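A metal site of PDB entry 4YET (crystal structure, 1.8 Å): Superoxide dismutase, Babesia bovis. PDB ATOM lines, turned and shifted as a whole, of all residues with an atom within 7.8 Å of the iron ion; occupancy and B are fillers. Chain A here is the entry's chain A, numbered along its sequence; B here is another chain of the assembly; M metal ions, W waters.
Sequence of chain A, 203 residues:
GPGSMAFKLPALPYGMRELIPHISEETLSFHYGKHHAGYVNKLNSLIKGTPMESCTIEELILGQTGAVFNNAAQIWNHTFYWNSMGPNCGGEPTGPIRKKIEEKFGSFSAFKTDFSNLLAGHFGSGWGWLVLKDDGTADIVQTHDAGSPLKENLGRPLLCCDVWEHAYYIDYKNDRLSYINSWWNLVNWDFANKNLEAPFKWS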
ATOM      1  N   HIS A  31       6.533   6.755 -12.922  1.00  0.00           N
ATOM      2  CA  HIS A  31       5.803   7.087 -11.718  1.00  0.00           C
ATOM      3  C   HIS A  31       6.490   6.530 -10.464  1.00  0.00           C
ATOM      4  O   HIS A  31       6.685   7.243  -9.478  1.00  0.00           O
ATOM      5  CB  HIS A  31       4.360   6.565 -11.835  1.00  0.00           C
ATOM      6  CG  HIS A  31       3.420   7.226 -10.881  1.00  0.00           C
ATOM      7  ND1 HIS A  31       2.070   6.952 -10.868  1.00  0.00           N
ATOM      8  CD2 HIS A  31       3.622   8.172  -9.925  1.00  0.00           C
ATOM      9  CE1 HIS A  31       1.481   7.686  -9.945  1.00  0.00           C
ATOM     10  NE2 HIS A  31       2.396   8.436  -9.348  1.00  0.00           N
ATOM     11  N   TYR A  32       6.909   5.276 -10.526  1.00  0.00           N
ATOM     12  CA  TYR A  32       7.639   4.687  -9.410  1.00  0.00           C
ATOM     13  C   TYR A  32       9.118   5.067  -9.471  1.00  0.00           C
ATOM     14  O   TYR A  32       9.672   5.587  -8.496  1.00  0.00           O
ATOM     15  CB  TYR A  32       7.473   3.158  -9.412  1.00  0.00           C
ATOM     16  CG  TYR A  32       8.228   2.452  -8.314  1.00  0.00           C
ATOM     17  CD1 TYR A  32       7.756   2.441  -7.017  1.00  0.00           C
ATOM     18  CD2 TYR A  32       9.432   1.805  -8.590  1.00  0.00           C
ATOM     19  CE1 TYR A  32       8.459   1.779  -5.995  1.00  0.00           C
ATOM     20  CE2 TYR A  32      10.139   1.155  -7.607  1.00  0.00           C
ATOM     21  CZ  TYR A  32       9.641   1.142  -6.319  1.00  0.00           C
ATOM     22  OH  TYR A  32      10.370   0.481  -5.352  1.00  0.00           O
ATOM     23  N   HIS A  35       9.283   9.604 -10.087  1.00  0.00           N
ATOM     24  CA  HIS A  35       8.534  10.468  -9.147  1.00  0.00           C
ATOM     25  C   HIS A  35       8.660   9.976  -7.702  1.00  0.00           C
ATOM     26  O   HIS A  35       9.087  10.712  -6.825  1.00  0.00           O
ATOM     27  CB  HIS A  35       7.052  10.574  -9.531  1.00  0.00           C
ATOM     28  CG  HIS A  35       6.800  11.341 -10.790  1.00  0.00           C
ATOM     29  ND1 HIS A  35       6.752  12.720 -10.828  1.00  0.00           N
ATOM     30  CD2 HIS A  35       6.573  10.924 -12.054  1.00  0.00           C
ATOM     31  CE1 HIS A  35       6.511  13.114 -12.071  1.00  0.00           C
ATOM     32  NE2 HIS A  35       6.395  12.038 -12.835  1.00  0.00           N
ATOM     33  N   HIS A  36       8.272   8.733  -7.462  1.00  0.00           N
ATOM     34  CA  HIS A  36       8.288   8.201  -6.103  1.00  0.00           C
ATOM     35  C   HIS A  36       9.719   8.166  -5.566  1.00  0.00           C
ATOM     36  O   HIS A  36       9.970   8.602  -4.461  1.00  0.00           O
ATOM     37  CB  HIS A  36       7.646   6.813  -6.066  1.00  0.00           C
ATOM     38  CG  HIS A  36       7.247   6.360  -4.699  1.00  0.00           C
ATOM     39  ND1 HIS A  36       6.631   5.143  -4.480  1.00  0.00           N
ATOM     40  CD2 HIS A  36       7.361   6.962  -3.479  1.00  0.00           C
ATOM     41  CE1 HIS A  36       6.389   5.009  -3.185  1.00  0.00           C
ATOM     42  NE2 HIS A  36       6.809   6.091  -2.562  1.00  0.00           N
ATOM     43  N   TYR A  39      10.837  11.598  -4.508  1.00  0.00           N
ATOM     44  CA  TYR A  39      10.373  12.095  -3.202  1.00  0.00           C
ATOM     45  C   TYR A  39      11.247  11.536  -2.075  1.00  0.00           C
ATOM     46  O   TYR A  39      11.549  12.233  -1.087  1.00  0.00           O
ATOM     47  CB  TYR A  39       8.920  11.715  -2.961  1.00  0.00           C
ATOM     48  CG  TYR A  39       7.932  12.412  -3.883  1.00  0.00           C
ATOM     49  CD1 TYR A  39       7.843  13.797  -3.893  1.00  0.00           C
ATOM     50  CD2 TYR A  39       7.094  11.688  -4.728  1.00  0.00           C
ATOM     51  CE1 TYR A  39       6.947  14.454  -4.726  1.00  0.00           C
ATOM     52  CE2 TYR A  39       6.195  12.338  -5.573  1.00  0.00           C
ATOM     53  CZ  TYR A  39       6.126  13.723  -5.554  1.00  0.00           C
ATOM     54  OH  TYR A  39       5.233  14.406  -6.361  1.00  0.00           O
ATOM     55  N   GLN A  74       3.992  12.536   0.118  1.00  0.00           N
ATOM     56  CA  GLN A  74       3.969  11.876  -1.196  1.00  0.00           C
ATOM     57  C   GLN A  74       4.620  10.502  -1.143  1.00  0.00           C
ATOM     58  O   GLN A  74       4.191   9.581  -1.821  1.00  0.00           O
ATOM     59  CB  GLN A  74       4.639  12.738  -2.255  1.00  0.00           C
ATOM     60  CG  GLN A  74       3.817  13.962  -2.664  1.00  0.00           C
ATOM     61  CD  GLN A  74       2.525  13.586  -3.370  1.00  0.00           C
ATOM     62  OE1 GLN A  74       1.526  13.262  -2.722  1.00  0.00           O
ATOM     63  NE2 GLN A  74       2.525  13.666  -4.691  1.00  0.00           N
ATOM     64  N   ASN A  77       1.844   8.399   0.486  1.00  0.00           N
ATOM     65  CA  ASN A  77       0.701   8.297  -0.429  1.00  0.00           C
ATOM     66  C   ASN A  77       0.991   7.338  -1.603  1.00  0.00           C
ATOM     67  O   ASN A  77       0.134   6.515  -1.967  1.00  0.00           O
ATOM     68  CB  ASN A  77       0.340   9.682  -0.968  1.00  0.00           C
ATOM     69  CG  ASN A  77      -0.228  10.604   0.106  1.00  0.00           C
ATOM     70  OD1 ASN A  77      -0.606  10.166   1.195  1.00  0.00           O
ATOM     71  ND2 ASN A  77      -0.295  11.887  -0.219  1.00  0.00           N
ATOM     72  N   HIS A  78       2.189   7.420  -2.164  1.00  0.00           N
ATOM     73  CA  HIS A  78       2.531   6.562  -3.295  1.00  0.00           C
ATOM     74  C   HIS A  78       2.661   5.113  -2.876  1.00  0.00           C
ATOM     75  O   HIS A  78       2.165   4.221  -3.563  1.00  0.00           O
ATOM     76  CB  HIS A  78       3.802   7.060  -4.008  1.00  0.00           C
ATOM     77  CG  HIS A  78       3.529   8.239  -4.897  1.00  0.00           C
ATOM     78  ND1 HIS A  78       3.500   9.540  -4.418  1.00  0.00           N
ATOM     79  CD2 HIS A  78       3.184   8.312  -6.198  1.00  0.00           C
ATOM     80  CE1 HIS A  78       3.192  10.359  -5.400  1.00  0.00           C
ATOM     81  NE2 HIS A  78       2.974   9.639  -6.491  1.00  0.00           N
ATOM     82  N   TYR A  81      -0.741   3.877  -2.598  1.00  0.00           N
ATOM     83  CA  TYR A  81      -1.266   3.713  -3.951  1.00  0.00           C
ATOM     84  C   TYR A  81      -0.836   2.421  -4.632  1.00  0.00           C
ATOM     85  O   TYR A  81      -1.673   1.692  -5.200  1.00  0.00           O
ATOM     86  CB  TYR A  81      -0.839   4.930  -4.766  1.00  0.00           C
ATOM     87  CG  TYR A  81      -1.168   4.929  -6.242  1.00  0.00           C
ATOM     88  CD1 TYR A  81      -2.492   4.911  -6.686  1.00  0.00           C
ATOM     89  CD2 TYR A  81      -0.149   4.999  -7.185  1.00  0.00           C
ATOM     90  CE1 TYR A  81      -2.788   4.945  -8.050  1.00  0.00           C
ATOM     91  CE2 TYR A  81      -0.433   5.035  -8.545  1.00  0.00           C
ATOM     92  CZ  TYR A  81      -1.763   5.013  -8.970  1.00  0.00           C
ATOM     93  OH  TYR A  81      -2.027   5.058 -10.321  1.00  0.00           O
ATOM     94  N   TRP A  82       0.455   2.087  -4.569  1.00  0.00           N
ATOM     95  CA  TRP A  82       0.895   0.825  -5.179  1.00  0.00           C
ATOM     96  C   TRP A  82       0.210  -0.363  -4.533  1.00  0.00           C
ATOM     97  O   TRP A  82      -0.172  -1.312  -5.232  1.00  0.00           O
ATOM     98  CB  TRP A  82       2.410   0.645  -5.103  1.00  0.00           C
ATOM     99  CG  TRP A  82       3.182   1.819  -5.647  1.00  0.00           C
ATOM    100  CD1 TRP A  82       4.176   2.502  -5.001  1.00  0.00           C
ATOM    101  CD2 TRP A  82       3.017   2.448  -6.927  1.00  0.00           C
ATOM    102  NE1 TRP A  82       4.640   3.516  -5.810  1.00  0.00           N
ATOM    103  CE2 TRP A  82       3.941   3.521  -6.986  1.00  0.00           C
ATOM    104  CE3 TRP A  82       2.180   2.221  -8.022  1.00  0.00           C
ATOM    105  CZ2 TRP A  82       4.061   4.352  -8.098  1.00  0.00           C
ATOM    106  CZ3 TRP A  82       2.298   3.047  -9.146  1.00  0.00           C
ATOM    107  CH2 TRP A  82       3.233   4.110  -9.170  1.00  0.00           C
ATOM    108  N   GLY A 126      -4.012  15.820  -7.048  1.00  0.00           N
ATOM    109  CA  GLY A 126      -4.559  15.338  -5.788  1.00  0.00           C
ATOM    110  C   GLY A 126      -4.804  13.853  -5.747  1.00  0.00           C
ATOM    111  O   GLY A 126      -4.288  13.117  -6.589  1.00  0.00           O
ATOM    112  N   TRP A 127      -5.589  13.428  -4.763  1.00  0.00           N
ATOM    113  CA  TRP A 127      -5.790  12.022  -4.376  1.00  0.00           C
ATOM    114  C   TRP A 127      -7.245  11.779  -4.010  1.00  0.00           C
ATOM    115  O   TRP A 127      -7.857  12.626  -3.388  1.00  0.00           O
ATOM    116  CB  TRP A 127      -4.930  11.653  -3.164  1.00  0.00           C
ATOM    117  CG  TRP A 127      -3.485  11.835  -3.360  1.00  0.00           C
ATOM    118  CD1 TRP A 127      -2.744  12.986  -3.193  1.00  0.00           C
ATOM    119  CD2 TRP A 127      -2.551  10.826  -3.767  1.00  0.00           C
ATOM    120  NE1 TRP A 127      -1.423  12.739  -3.470  1.00  0.00           N
ATOM    121  CE2 TRP A 127      -1.272  11.425  -3.824  1.00  0.00           C
ATOM    122  CE3 TRP A 127      -2.674   9.469  -4.082  1.00  0.00           C
ATOM    123  CZ2 TRP A 127      -0.133  10.724  -4.203  1.00  0.00           C
ATOM    124  CZ3 TRP A 127      -1.520   8.760  -4.437  1.00  0.00           C
ATOM    125  CH2 TRP A 127      -0.278   9.391  -4.501  1.00  0.00           C
ATOM    126  N   ASP A 162      -4.390   7.901  -7.143  1.00  0.00           N
ATOM    127  CA  ASP A 162      -3.629   9.108  -7.516  1.00  0.00           C
ATOM    128  C   ASP A 162      -4.251   9.764  -8.745  1.00  0.00           C
ATOM    129  O   ASP A 162      -4.414   9.094  -9.767  1.00  0.00           O
ATOM    130  CB  ASP A 162      -2.180   8.683  -7.794  1.00  0.00           C
ATOM    131  CG  ASP A 162      -1.210   9.853  -7.984  1.00  0.00           C
ATOM    132  OD1 ASP A 162      -1.603  11.031  -7.848  1.00  0.00           O
ATOM    133  OD2 ASP A 162      -0.025   9.565  -8.227  1.00  0.00           O
ATOM    134  N   VAL A 163      -4.587  11.054  -8.671  1.00  0.00           N
ATOM    135  CA  VAL A 163      -5.085  11.717  -9.889  1.00  0.00           C
ATOM    136  C   VAL A 163      -4.217  12.901 -10.282  1.00  0.00           C
ATOM    137  O   VAL A 163      -4.643  13.724 -11.080  1.00  0.00           O
ATOM    138  CB  VAL A 163      -6.582  12.123  -9.768  1.00  0.00           C
ATOM    139  CG1 VAL A 163      -7.462  10.845  -9.680  1.00  0.00           C
ATOM    140  CG2 VAL A 163      -6.839  13.057  -8.597  1.00  0.00           C
ATOM    141  N   TRP A 164      -2.997  12.978  -9.749  1.00  0.00           N
ATOM    142  CA  TRP A 164      -1.972  13.789 -10.374  1.00  0.00           C
ATOM    143  C   TRP A 164      -1.890  13.370 -11.831  1.00  0.00           C
ATOM    144  O   TRP A 164      -2.000  12.165 -12.153  1.00  0.00           O
ATOM    145  CB  TRP A 164      -0.594  13.601  -9.717  1.00  0.00           C
ATOM    146  CG  TRP A 164      -0.411  14.308  -8.395  1.00  0.00           C
ATOM    147  CD1 TRP A 164      -1.110  14.119  -7.242  1.00  0.00           C
ATOM    148  CD2 TRP A 164       0.597  15.271  -8.110  1.00  0.00           C
ATOM    149  NE1 TRP A 164      -0.604  14.932  -6.244  1.00  0.00           N
ATOM    150  CE2 TRP A 164       0.449  15.650  -6.755  1.00  0.00           C
ATOM    151  CE3 TRP A 164       1.593  15.871  -8.881  1.00  0.00           C
ATOM    152  CZ2 TRP A 164       1.278  16.596  -6.149  1.00  0.00           C
ATOM    153  CZ3 TRP A 164       2.433  16.812  -8.283  1.00  0.00           C
ATOM    154  CH2 TRP A 164       2.264  17.167  -6.927  1.00  0.00           C
ATOM    155  N   GLU A 165      -1.644  14.330 -12.712  1.00  0.00           N
ATOM    156  CA  GLU A 165      -1.633  14.006 -14.139  1.00  0.00           C
ATOM    157  C   GLU A 165      -0.536  13.006 -14.521  1.00  0.00           C
ATOM    158  O   GLU A 165      -0.759  12.189 -15.424  1.00  0.00           O
ATOM    159  CB  GLU A 165      -1.495  15.285 -14.980  1.00  0.00           C
ATOM    160  CG  GLU A 165      -2.779  16.099 -14.965  1.00  0.00           C
ATOM    161  CD  GLU A 165      -2.725  17.385 -15.759  1.00  0.00           C
ATOM    162  OE1 GLU A 165      -1.676  18.084 -15.721  1.00  0.00           O
ATOM    163  OE2 GLU A 165      -3.756  17.700 -16.408  1.00  0.00           O
ATOM    164  N   HIS A 166       0.610  13.023 -13.829  1.00  0.00           N
ATOM    165  CA  HIS A 166       1.649  12.038 -14.134  1.00  0.00           C
ATOM    166  C   HIS A 166       1.205  10.589 -13.899  1.00  0.00           C
ATOM    167  O   HIS A 166       1.822   9.677 -14.433  1.00  0.00           O
ATOM    168  CB  HIS A 166       2.952  12.292 -13.345  1.00  0.00           C
ATOM    169  CG  HIS A 166       2.823  12.137 -11.855  1.00  0.00           C
ATOM    170  ND1 HIS A 166       3.039  13.186 -10.986  1.00  0.00           N
ATOM    171  CD2 HIS A 166       2.569  11.045 -11.091  1.00  0.00           C
ATOM    172  CE1 HIS A 166       2.869  12.751  -9.740  1.00  0.00           C
ATOM    173  NE2 HIS A 166       2.592  11.456  -9.780  1.00  0.00           N
ATOM    174  N   ALA A 167       0.152  10.360 -13.118  1.00  0.00           N
ATOM    175  CA  ALA A 167      -0.326   8.999 -12.873  1.00  0.00           C
ATOM    176  C   ALA A 167      -0.920   8.394 -14.118  1.00  0.00           C
ATOM    177  O   ALA A 167      -0.978   7.176 -14.242  1.00  0.00           O
ATOM    178  CB  ALA A 167      -1.352   8.968 -11.746  1.00  0.00           C
ATOM    179  N   TYR A 168      -1.407   9.226 -15.021  1.00  0.00           N
ATOM    180  CA  TYR A 168      -2.120   8.691 -16.180  1.00  0.00           C
ATOM    181  C   TYR A 168      -1.767   9.281 -17.534  1.00  0.00           C
ATOM    182  O   TYR A 168      -2.242   8.775 -18.565  1.00  0.00           O
ATOM    183  CB  TYR A 168      -3.630   8.829 -15.962  1.00  0.00           C
ATOM    184  CG  TYR A 168      -4.155  10.239 -15.722  1.00  0.00           C
ATOM    185  CD1 TYR A 168      -4.478  11.078 -16.793  1.00  0.00           C
ATOM    186  CD2 TYR A 168      -4.387  10.706 -14.426  1.00  0.00           C
ATOM    187  CE1 TYR A 168      -4.998  12.363 -16.579  1.00  0.00           C
ATOM    188  CE2 TYR A 168      -4.888  11.999 -14.205  1.00  0.00           C
ATOM    189  CZ  TYR A 168      -5.208  12.811 -15.278  1.00  0.00           C
ATOM    190  OH  TYR A 168      -5.729  14.075 -15.079  1.00  0.00           O
ATOM    191  N   TYR A 179      -8.616   6.413 -17.357  1.00  0.00           N
ATOM    192  CA  TYR A 179      -7.692   5.978 -16.335  1.00  0.00           C
ATOM    193  C   TYR A 179      -8.453   5.459 -15.100  1.00  0.00           C
ATOM    194  O   TYR A 179      -8.125   4.413 -14.547  1.00  0.00           O
ATOM    195  CB  TYR A 179      -6.791   7.139 -15.942  1.00  0.00           C
ATOM    196  CG  TYR A 179      -6.108   6.958 -14.594  1.00  0.00           C
ATOM    197  CD1 TYR A 179      -5.110   6.006 -14.407  1.00  0.00           C
ATOM    198  CD2 TYR A 179      -6.418   7.804 -13.528  1.00  0.00           C
ATOM    199  CE1 TYR A 179      -4.466   5.874 -13.172  1.00  0.00           C
ATOM    200  CE2 TYR A 179      -5.782   7.679 -12.295  1.00  0.00           C
ATOM    201  CZ  TYR A 179      -4.821   6.695 -12.124  1.00  0.00           C
ATOM    202  OH  TYR A 179      -4.177   6.613 -10.882  1.00  0.00           O
ATOM    203  N   GLU B 165       1.374  19.490 -15.253  1.00  0.00           N
ATOM    204  CA  GLU B 165       2.126  18.402 -15.872  1.00  0.00           C
ATOM    205  C   GLU B 165       1.710  18.167 -17.325  1.00  0.00           C
ATOM    206  O   GLU B 165       2.554  17.783 -18.156  1.00  0.00           O
ATOM    207  CB  GLU B 165       1.979  17.109 -15.046  1.00  0.00           C
ATOM    208  CG  GLU B 165       2.737  17.260 -13.711  1.00  0.00           C
ATOM    209  CD  GLU B 165       2.641  16.030 -12.806  1.00  0.00           C
ATOM    210  OE1 GLU B 165       1.530  15.457 -12.678  1.00  0.00           O
ATOM    211  OE2 GLU B 165       3.680  15.669 -12.193  1.00  0.00           O
HETATM  212 FE    FE M   1       1.847  10.229  -8.232  1.00  0.00          FE
HETATM  213  O   HOH W   1       1.149  12.005  -7.116  1.00  0.00           O
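The iron ion is bound by the side-chain carboxylate of Asp 162 (2.0 Å), a ring nitrogen (NE2) of His 166 (2.1 Å), a ring nitrogen (NE2) of His 78 (2.2 Å), a ring nitrogen (NE2) of His 31 (2.2 Å) and water W1 (2.2 Å).
The nearest printed residue that does not touch the iron ion is Trp 127 (4.4 Å).
The side-chain carboxylate of Asp 162 is in hydrogen-bond range of the backbone NH of Trp 164 (3.1 Å).
O of Asp 162 sits at hydrogen-bond distance from OH of Tyr 179.
OE2 of Glu 165 of chain B sits at hydrogen-bond distance from ND1 of His 166 (2.8 Å).
O of Gln 74 sits at hydrogen-bond distance from ND1 of His 78, at 2.7 Å.
The backbone carbonyl oxygen of His 78 sits close to the indole nitrogen of Trp 82 (3.4 Å).
The backbone NH (N) of His 36 is in hydrogen-bond range of the backbone carbonyl oxygen (O) of His 31.
Water W1 lies within hydrogen-bond range of the side-chain carboxylate (OD1) of Asp 162 (3.0 Å) and the side-chain amide nitrogen (NE2) of Gln 74 (3.2 Å).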
